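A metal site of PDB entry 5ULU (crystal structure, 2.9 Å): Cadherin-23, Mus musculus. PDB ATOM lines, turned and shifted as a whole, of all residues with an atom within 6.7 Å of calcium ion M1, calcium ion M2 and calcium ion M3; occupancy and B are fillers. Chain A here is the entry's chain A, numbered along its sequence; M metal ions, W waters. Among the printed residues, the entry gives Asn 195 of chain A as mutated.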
ATOM      1  N   GLU A  17      -7.512   2.957 -24.957  1.00  0.00           N
ATOM      2  CA  GLU A  17      -6.879   1.867 -24.204  1.00  0.00           C
ATOM      3  C   GLU A  17      -6.732   0.630 -25.084  1.00  0.00           C
ATOM      4  O   GLU A  17      -7.502   0.431 -26.040  1.00  0.00           O
ATOM      5  CB  GLU A  17      -7.642   1.528 -22.898  1.00  0.00           C
ATOM      6  CG  GLU A  17      -9.128   1.233 -23.011  1.00  0.00           C
ATOM      7  CD  GLU A  17      -9.692   0.422 -21.835  1.00  0.00           C
ATOM      8  OE1 GLU A  17     -10.924   0.540 -21.601  1.00  0.00           O
ATOM      9  OE2 GLU A  17      -8.935  -0.346 -21.176  1.00  0.00           O
ATOM     10  N   ASN A  18      -5.705  -0.170 -24.800  1.00  0.00           N
ATOM     11  CA  ASN A  18      -5.421  -1.421 -25.543  1.00  0.00           C
ATOM     12  C   ASN A  18      -4.821  -1.208 -26.927  1.00  0.00           C
ATOM     13  O   ASN A  18      -4.460  -2.195 -27.559  1.00  0.00           O
ATOM     14  CB  ASN A  18      -6.663  -2.337 -25.670  1.00  0.00           C
ATOM     15  CG  ASN A  18      -7.275  -2.705 -24.336  1.00  0.00           C
ATOM     16  OD1 ASN A  18      -6.589  -3.201 -23.457  1.00  0.00           O
ATOM     17  ND2 ASN A  18      -8.592  -2.470 -24.178  1.00  0.00           N
ATOM     18  N   ILE A  74      -1.974  -0.658 -22.238  1.00  0.00           N
ATOM     19  CA  ILE A  74      -2.623   0.544 -21.684  1.00  0.00           C
ATOM     20  C   ILE A  74      -4.085   0.270 -21.283  1.00  0.00           C
ATOM     21  O   ILE A  74      -4.989   0.309 -22.119  1.00  0.00           O
ATOM     22  CB  ILE A  74      -2.557   1.714 -22.695  1.00  0.00           C
ATOM     23  CG1 ILE A  74      -1.104   2.018 -23.056  1.00  0.00           C
ATOM     24  CG2 ILE A  74      -3.227   2.968 -22.127  1.00  0.00           C
ATOM     25  CD1 ILE A  74      -0.944   3.196 -24.000  1.00  0.00           C
ATOM     26  N   ASP A  75      -4.294   0.042 -19.986  1.00  0.00           N
ATOM     27  CA  ASP A  75      -5.611  -0.241 -19.406  1.00  0.00           C
ATOM     28  C   ASP A  75      -6.207   1.029 -18.758  1.00  0.00           C
ATOM     29  O   ASP A  75      -5.739   1.453 -17.710  1.00  0.00           O
ATOM     30  CB  ASP A  75      -5.464  -1.364 -18.364  1.00  0.00           C
ATOM     31  CG  ASP A  75      -6.796  -1.813 -17.781  1.00  0.00           C
ATOM     32  OD1 ASP A  75      -7.814  -1.166 -18.006  1.00  0.00           O
ATOM     33  OD2 ASP A  75      -6.818  -2.848 -17.106  1.00  0.00           O
ATOM     34  N   ARG A  76      -7.260   1.604 -19.353  1.00  0.00           N
ATOM     35  CA  ARG A  76      -7.986   2.704 -18.743  1.00  0.00           C
ATOM     36  C   ARG A  76      -8.451   2.363 -17.333  1.00  0.00           C
ATOM     37  O   ARG A  76      -8.397   3.193 -16.442  1.00  0.00           O
ATOM     38  CB  ARG A  76      -9.210   3.101 -19.544  1.00  0.00           C
ATOM     39  CG  ARG A  76      -9.673   4.523 -19.205  1.00  0.00           C
ATOM     40  CD  ARG A  76     -11.122   4.839 -19.549  1.00  0.00           C
ATOM     41  NE  ARG A  76     -12.042   3.934 -18.878  1.00  0.00           N
ATOM     42  CZ  ARG A  76     -12.415   4.013 -17.598  1.00  0.00           C
ATOM     43  NH1 ARG A  76     -11.930   4.970 -16.804  1.00  0.00           N
ATOM     44  NH2 ARG A  76     -13.259   3.117 -17.103  1.00  0.00           N
ATOM     45  N   GLU A  77      -8.886   1.127 -17.134  1.00  0.00           N
ATOM     46  CA  GLU A  77      -9.377   0.674 -15.837  1.00  0.00           C
ATOM     47  C   GLU A  77      -8.299   0.673 -14.721  1.00  0.00           C
ATOM     48  O   GLU A  77      -8.614   0.500 -13.569  1.00  0.00           O
ATOM     49  CB  GLU A  77     -10.027  -0.714 -15.978  1.00  0.00           C
ATOM     50  CG  GLU A  77     -11.444  -0.705 -16.556  1.00  0.00           C
ATOM     51  CD  GLU A  77     -11.563  -0.139 -17.964  1.00  0.00           C
ATOM     52  OE1 GLU A  77     -12.349   0.812 -18.142  1.00  0.00           O
ATOM     53  OE2 GLU A  77     -10.903  -0.653 -18.919  1.00  0.00           O
ATOM     54  N   ALA A  78      -7.033   0.849 -15.097  1.00  0.00           N
ATOM     55  CA  ALA A  78      -5.919   0.921 -14.147  1.00  0.00           C
ATOM     56  C   ALA A  78      -5.419   2.344 -13.851  1.00  0.00           C
ATOM     57  O   ALA A  78      -4.453   2.495 -13.132  1.00  0.00           O
ATOM     58  CB  ALA A  78      -4.765   0.070 -14.666  1.00  0.00           C
ATOM     59  N   LEU A 107      -9.000   7.006 -23.602  1.00  0.00           N
ATOM     60  CA  LEU A 107     -10.384   6.679 -23.925  1.00  0.00           C
ATOM     61  C   LEU A 107     -10.778   5.228 -23.565  1.00  0.00           C
ATOM     62  O   LEU A 107      -9.906   4.308 -23.534  1.00  0.00           O
ATOM     63  CB  LEU A 107     -10.664   6.962 -25.394  1.00  0.00           C
ATOM     64  CG  LEU A 107     -10.567   8.433 -25.801  1.00  0.00           C
ATOM     65  CD1 LEU A 107     -10.558   8.526 -27.316  1.00  0.00           C
ATOM     66  CD2 LEU A 107     -11.680   9.303 -25.193  1.00  0.00           C
ATOM     67  N   ASP A 108     -12.083   5.040 -23.312  1.00  0.00           N
ATOM     68  CA  ASP A 108     -12.608   3.790 -22.768  1.00  0.00           C
ATOM     69  C   ASP A 108     -12.998   2.804 -23.880  1.00  0.00           C
ATOM     70  O   ASP A 108     -13.634   3.149 -24.884  1.00  0.00           O
ATOM     71  CB  ASP A 108     -13.804   4.084 -21.854  1.00  0.00           C
ATOM     72  CG  ASP A 108     -14.355   2.833 -21.177  1.00  0.00           C
ATOM     73  OD1 ASP A 108     -13.568   1.931 -20.812  1.00  0.00           O
ATOM     74  OD2 ASP A 108     -15.597   2.786 -20.981  1.00  0.00           O
ATOM     75  N   ASP A 109     -12.592   1.569 -23.667  1.00  0.00           N
ATOM     76  CA  ASP A 109     -12.984   0.448 -24.480  1.00  0.00           C
ATOM     77  C   ASP A 109     -13.991  -0.332 -23.679  1.00  0.00           C
ATOM     78  O   ASP A 109     -13.912  -0.364 -22.453  1.00  0.00           O
ATOM     79  CB  ASP A 109     -11.756  -0.419 -24.732  1.00  0.00           C
ATOM     80  CG  ASP A 109     -11.797  -1.145 -26.032  1.00  0.00           C
ATOM     81  OD1 ASP A 109     -12.547  -0.683 -26.910  1.00  0.00           O
ATOM     82  OD2 ASP A 109     -11.052  -2.147 -26.174  1.00  0.00           O
ATOM     83  N   ASN A 110     -14.962  -0.969 -24.339  1.00  0.00           N
ATOM     84  CA  ASN A 110     -15.856  -1.881 -23.621  1.00  0.00           C
ATOM     85  C   ASN A 110     -15.191  -3.256 -23.529  1.00  0.00           C
ATOM     86  O   ASN A 110     -15.516  -4.188 -24.283  1.00  0.00           O
ATOM     87  CB  ASN A 110     -17.243  -1.953 -24.254  1.00  0.00           C
ATOM     88  CG  ASN A 110     -18.284  -2.531 -23.310  1.00  0.00           C
ATOM     89  OD1 ASN A 110     -17.998  -2.742 -22.121  1.00  0.00           O
ATOM     90  ND2 ASN A 110     -19.487  -2.782 -23.817  1.00  0.00           N
ATOM     91  N   ASP A 111     -14.258  -3.375 -22.576  1.00  0.00           N
ATOM     92  CA  ASP A 111     -13.509  -4.622 -22.388  1.00  0.00           C
ATOM     93  C   ASP A 111     -13.788  -5.302 -21.038  1.00  0.00           C
ATOM     94  O   ASP A 111     -12.977  -6.100 -20.527  1.00  0.00           O
ATOM     95  CB  ASP A 111     -12.014  -4.413 -22.641  1.00  0.00           C
ATOM     96  CG  ASP A 111     -11.429  -3.261 -21.878  1.00  0.00           C
ATOM     97  OD1 ASP A 111     -12.099  -2.671 -20.997  1.00  0.00           O
ATOM     98  OD2 ASP A 111     -10.269  -2.955 -22.165  1.00  0.00           O
ATOM     99  N   ASN A 112     -14.975  -5.035 -20.499  1.00  0.00           N
ATOM    100  CA  ASN A 112     -15.382  -5.647 -19.274  1.00  0.00           C
ATOM    101  C   ASN A 112     -16.867  -6.023 -19.354  1.00  0.00           C
ATOM    102  O   ASN A 112     -17.720  -5.174 -19.657  1.00  0.00           O
ATOM    103  CB  ASN A 112     -15.095  -4.707 -18.067  1.00  0.00           C
ATOM    104  CG  ASN A 112     -13.604  -4.524 -17.806  1.00  0.00           C
ATOM    105  OD1 ASN A 112     -12.965  -5.404 -17.259  1.00  0.00           O
ATOM    106  ND2 ASN A 112     -13.039  -3.414 -18.273  1.00  0.00           N
ATOM    107  N   TRP A 113     -17.153  -7.288 -19.056  1.00  0.00           N
ATOM    108  CA  TRP A 113     -18.489  -7.833 -19.212  1.00  0.00           C
ATOM    109  C   TRP A 113     -19.304  -7.483 -17.976  1.00  0.00           C
ATOM    110  O   TRP A 113     -18.792  -7.553 -16.867  1.00  0.00           O
ATOM    111  CB  TRP A 113     -18.441  -9.338 -19.355  1.00  0.00           C
ATOM    112  CG  TRP A 113     -18.217  -9.807 -20.722  1.00  0.00           C
ATOM    113  CD1 TRP A 113     -19.113 -10.494 -21.516  1.00  0.00           C
ATOM    114  CD2 TRP A 113     -17.030  -9.678 -21.483  1.00  0.00           C
ATOM    115  NE1 TRP A 113     -18.545 -10.756 -22.735  1.00  0.00           N
ATOM    116  CE2 TRP A 113     -17.268 -10.281 -22.733  1.00  0.00           C
ATOM    117  CE3 TRP A 113     -15.790  -9.093 -21.238  1.00  0.00           C
ATOM    118  CZ2 TRP A 113     -16.309 -10.330 -23.729  1.00  0.00           C
ATOM    119  CZ3 TRP A 113     -14.846  -9.127 -22.226  1.00  0.00           C
ATOM    120  CH2 TRP A 113     -15.096  -9.747 -23.451  1.00  0.00           C
ATOM    121  N   PRO A 114     -20.577  -7.112 -18.154  1.00  0.00           N
ATOM    122  CA  PRO A 114     -21.496  -7.165 -17.016  1.00  0.00           C
ATOM    123  C   PRO A 114     -21.388  -8.459 -16.211  1.00  0.00           C
ATOM    124  O   PRO A 114     -21.559  -9.560 -16.763  1.00  0.00           O
ATOM    125  CB  PRO A 114     -22.874  -7.065 -17.674  1.00  0.00           C
ATOM    126  CG  PRO A 114     -22.626  -6.795 -19.137  1.00  0.00           C
ATOM    127  CD  PRO A 114     -21.189  -6.440 -19.306  1.00  0.00           C
ATOM    128  N   ASP A 142     -19.902  -3.587 -13.702  1.00  0.00           N
ATOM    129  CA  ASP A 142     -19.182  -3.421 -14.956  1.00  0.00           C
ATOM    130  C   ASP A 142     -18.092  -2.376 -14.732  1.00  0.00           C
ATOM    131  O   ASP A 142     -18.384  -1.232 -14.459  1.00  0.00           O
ATOM    132  CB  ASP A 142     -20.167  -2.957 -16.051  1.00  0.00           C
ATOM    133  CG  ASP A 142     -19.567  -2.953 -17.487  1.00  0.00           C
ATOM    134  OD1 ASP A 142     -18.495  -2.362 -17.778  1.00  0.00           O
ATOM    135  OD2 ASP A 142     -20.212  -3.523 -18.371  1.00  0.00           O
ATOM    136  N   GLU A 143     -16.847  -2.778 -14.916  1.00  0.00           N
ATOM    137  CA  GLU A 143     -15.724  -1.913 -14.624  1.00  0.00           C
ATOM    138  C   GLU A 143     -15.441  -0.810 -15.656  1.00  0.00           C
ATOM    139  O   GLU A 143     -14.460  -0.094 -15.528  1.00  0.00           O
ATOM    140  CB  GLU A 143     -14.468  -2.765 -14.370  1.00  0.00           C
ATOM    141  CG  GLU A 143     -14.615  -3.758 -13.200  1.00  0.00           C
ATOM    142  CD  GLU A 143     -14.865  -3.098 -11.821  1.00  0.00           C
ATOM    143  OE1 GLU A 143     -14.062  -2.237 -11.406  1.00  0.00           O
ATOM    144  OE2 GLU A 143     -15.858  -3.475 -11.141  1.00  0.00           O
ATOM    145  N   ASP A 144     -16.281  -0.628 -16.666  1.00  0.00           N
ATOM    146  CA  ASP A 144     -16.047   0.444 -17.649  1.00  0.00           C
ATOM    147  C   ASP A 144     -16.773   1.723 -17.233  1.00  0.00           C
ATOM    148  O   ASP A 144     -17.423   1.777 -16.179  1.00  0.00           O
ATOM    149  CB  ASP A 144     -16.507  -0.014 -19.040  1.00  0.00           C
ATOM    150  CG  ASP A 144     -15.775  -1.253 -19.547  1.00  0.00           C
ATOM    151  OD1 ASP A 144     -14.538  -1.202 -19.719  1.00  0.00           O
ATOM    152  OD2 ASP A 144     -16.464  -2.267 -19.836  1.00  0.00           O
ATOM    153  N   SER A 145     -16.646   2.748 -18.080  1.00  0.00           N
ATOM    154  CA  SER A 145     -17.232   4.085 -17.838  1.00  0.00           C
ATOM    155  C   SER A 145     -18.160   4.500 -18.991  1.00  0.00           C
ATOM    156  O   SER A 145     -17.961   4.081 -20.156  1.00  0.00           O
ATOM    157  CB  SER A 145     -16.107   5.115 -17.714  1.00  0.00           C
ATOM    158  OG  SER A 145     -15.365   5.204 -18.929  1.00  0.00           O
ATOM    159  N   LEU A 147     -21.314   4.787 -21.522  1.00  0.00           N
ATOM    160  CA  LEU A 147     -22.084   3.766 -22.278  1.00  0.00           C
ATOM    161  C   LEU A 147     -21.602   2.353 -22.036  1.00  0.00           C
ATOM    162  O   LEU A 147     -22.405   1.445 -21.799  1.00  0.00           O
ATOM    163  CB  LEU A 147     -22.026   4.055 -23.792  1.00  0.00           C
ATOM    164  CG  LEU A 147     -22.838   5.286 -24.242  1.00  0.00           C
ATOM    165  CD1 LEU A 147     -22.159   6.022 -25.393  1.00  0.00           C
ATOM    166  CD2 LEU A 147     -24.282   4.895 -24.564  1.00  0.00           C
ATOM    167  N   ASN A 148     -20.277   2.182 -22.091  1.00  0.00           N
ATOM    168  CA  ASN A 148     -19.604   0.884 -21.878  1.00  0.00           C
ATOM    169  C   ASN A 148     -19.838   0.266 -20.476  1.00  0.00           C
ATOM    170  O   ASN A 148     -19.728  -0.961 -20.283  1.00  0.00           O
ATOM    171  CB  ASN A 148     -18.096   1.037 -22.086  1.00  0.00           C
ATOM    172  CG  ASN A 148     -17.735   1.452 -23.483  1.00  0.00           C
ATOM    173  OD1 ASN A 148     -18.578   1.504 -24.360  1.00  0.00           O
ATOM    174  ND2 ASN A 148     -16.453   1.754 -23.709  1.00  0.00           N
ATOM    175  N   GLY A 149     -20.120   1.110 -19.500  1.00  0.00           N
ATOM    176  CA  GLY A 149     -20.306   0.668 -18.137  1.00  0.00           C
ATOM    177  C   GLY A 149     -21.725   0.520 -17.673  1.00  0.00           C
ATOM    178  O   GLY A 149     -21.946  -0.026 -16.592  1.00  0.00           O
ATOM    179  N   GLU A 150     -22.694   1.036 -18.432  1.00  0.00           N
ATOM    180  CA  GLU A 150     -24.078   1.127 -17.913  1.00  0.00           C
ATOM    181  C   GLU A 150     -24.853  -0.129 -18.309  1.00  0.00           C
ATOM    182  O   GLU A 150     -24.408  -0.887 -19.156  1.00  0.00           O
ATOM    183  CB  GLU A 150     -24.785   2.457 -18.288  1.00  0.00           C
ATOM    184  CG  GLU A 150     -24.974   2.763 -19.764  1.00  0.00           C
ATOM    185  CD  GLU A 150     -25.587   4.139 -20.005  1.00  0.00           C
ATOM    186  OE1 GLU A 150     -26.649   4.420 -19.420  1.00  0.00           O
ATOM    187  OE2 GLU A 150     -25.013   4.935 -20.799  1.00  0.00           O
ATOM    188  N   ASN A 195     -24.664  -3.843 -21.733  1.00  0.00           N
ATOM    189  CA  ASN A 195     -24.084  -2.527 -21.935  1.00  0.00           C
ATOM    190  C   ASN A 195     -24.759  -1.886 -23.103  1.00  0.00           C
ATOM    191  O   ASN A 195     -25.295  -2.571 -23.972  1.00  0.00           O
ATOM    192  CB  ASN A 195     -22.576  -2.592 -22.217  1.00  0.00           C
ATOM    193  CG  ASN A 195     -21.760  -3.084 -21.033  1.00  0.00           C
ATOM    194  OD1 ASN A 195     -20.702  -3.707 -21.202  1.00  0.00           O
ATOM    195  ND2 ASN A 195     -22.225  -2.773 -19.809  1.00  0.00           N
ATOM    196  N   VAL A 199     -20.786  -1.994 -28.682  1.00  0.00           N
ATOM    197  CA  VAL A 199     -20.455  -3.362 -28.294  1.00  0.00           C
ATOM    198  C   VAL A 199     -21.320  -3.793 -27.096  1.00  0.00           C
ATOM    199  O   VAL A 199     -20.914  -3.616 -25.935  1.00  0.00           O
ATOM    200  CB  VAL A 199     -18.944  -3.487 -27.967  1.00  0.00           C
ATOM    201  CG1 VAL A 199     -18.592  -4.900 -27.557  1.00  0.00           C
ATOM    202  CG2 VAL A 199     -18.116  -3.080 -29.161  1.00  0.00           C
ATOM    203  N   LEU A 201     -22.132  -5.960 -24.652  1.00  0.00           N
ATOM    204  CA  LEU A 201     -21.776  -7.136 -23.866  1.00  0.00           C
ATOM    205  C   LEU A 201     -22.861  -7.369 -22.857  1.00  0.00           C
ATOM    206  O   LEU A 201     -23.394  -6.416 -22.320  1.00  0.00           O
ATOM    207  CB  LEU A 201     -20.469  -6.951 -23.116  1.00  0.00           C
ATOM    208  CG  LEU A 201     -19.219  -6.594 -23.899  1.00  0.00           C
ATOM    209  CD1 LEU A 201     -18.018  -6.572 -22.948  1.00  0.00           C
ATOM    210  CD2 LEU A 201     -19.025  -7.564 -25.048  1.00  0.00           C
HETATM  211 CA    CA M   1      -9.478  -2.256 -19.724  1.00  0.00          CA
HETATM  212 CA    CA M   2     -12.621  -0.172 -20.559  1.00  0.00          CA
HETATM  213 CA    CA M   3     -18.507  -3.149 -20.079  1.00  0.00          CA
HETATM  214  O   HOH W   1      -7.692  -2.573 -20.766  1.00  0.00           O
HETATM  215  O   HOH W   2     -10.514  -4.337 -19.003  1.00  0.00           O
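OD1 of Asn 110 is bound to calcium ion M3, 2.1 Å away.
O of Asn 112 is bound to calcium ion M3, 2.2 Å away.
Calcium ion M3 is bound by OD2 of Asp 144 (2.2 Å).
Calcium ion M3 is bound by OD1 of Asp 142 (2.4 Å).
OD2 of Asp 142 is bound to calcium ion M3, at 2.4 Å.
O of Asn 148 binds calcium ion M3.
OD1 of Asn 195 binds calcium ion M3 (2.5 Å).
Calcium ion M3 has seven donor atoms within binding distance.
Calcium ion M1 is bound by water W1 (2.1 Å), the side-chain carboxylate of Glu 77 (2.3 Å), water W2 (2.4 Å), the side-chain carboxylate of Glu 17 (2.5 Å), the side-chain carboxylate of Asp 75 (2.6 Å) and the side-chain carboxylate of Asp 111 (2.7 Å).
Calcium ion M1 has six donor atoms within binding distance.
Slightly farther from calcium ion M1 lies the side-chain carboxylate (OD1) of Asp 111 (2.9 Å).
Of the 26 residues printed, 6 come within 4 Å of calcium ion M3.
The side-chain carboxylate (OE1) of Glu 17 is bound to calcium ion M2.
O of Asp 109 is bound to calcium ion M2.
Calcium ion M2 is bound by the side-chain carboxylate (OD1) of Asp 108.
The side-chain carboxylate (OD1) of Asp 144 is bound to calcium ion M2, 2.3 Å away.
OE2 of Glu 77 binds calcium ion M2 (2.4 Å).
The side-chain carboxylate (OD1) of Asp 111 is bound to calcium ion M2 (2.6 Å).
Calcium ion M2 is bound by OE1 of Glu 77.
Water W2 lies within hydrogen-bond range of the side-chain amide nitrogen (ND2) of Asn 112 (2.8 Å) and the backbone carbonyl oxygen (O) of Asp 111 (3.4 Å).
The nearest printed residue that does not touch calcium ion M1 is Asn 112 (4.02 Å).
The backbone NH of Arg 76 lies close to the side-chain carboxylate of Glu 17 (3.2 Å).
The backbone NH of Asn 195 lies within hydrogen-bond range of the backbone carbonyl oxygen of Leu 201, at 2.9 Å.
The side-chain carboxylate (OD1) of Asp 108 lies close to the guanidinium group (NE) of Arg 76.
The backbone carbonyl oxygen (O) of Leu 107 is in hydrogen-bond range of the backbone NH (N) of Glu 17, at 3.1 Å.
The side-chain amide nitrogen of Asn 112 sits close to the side-chain carboxylate of Asp 111, at 3.0 Å.
The side-chain carboxylate of Asp 111 lies close to the side-chain amide nitrogen of Asn 18 (2.7 Å).
O of Val 199 is in hydrogen-bond range of ND2 of Asn 110 (2.7 Å).
OD2 of Asp 108 lies within hydrogen-bond range of ND2 of Asn 148 (3.0 Å).
Within 4 Å of calcium ion M2: Glu 17, Glu 77, Asp 108, Asp 109, Asp 111, Asn 112 and Asp 144.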
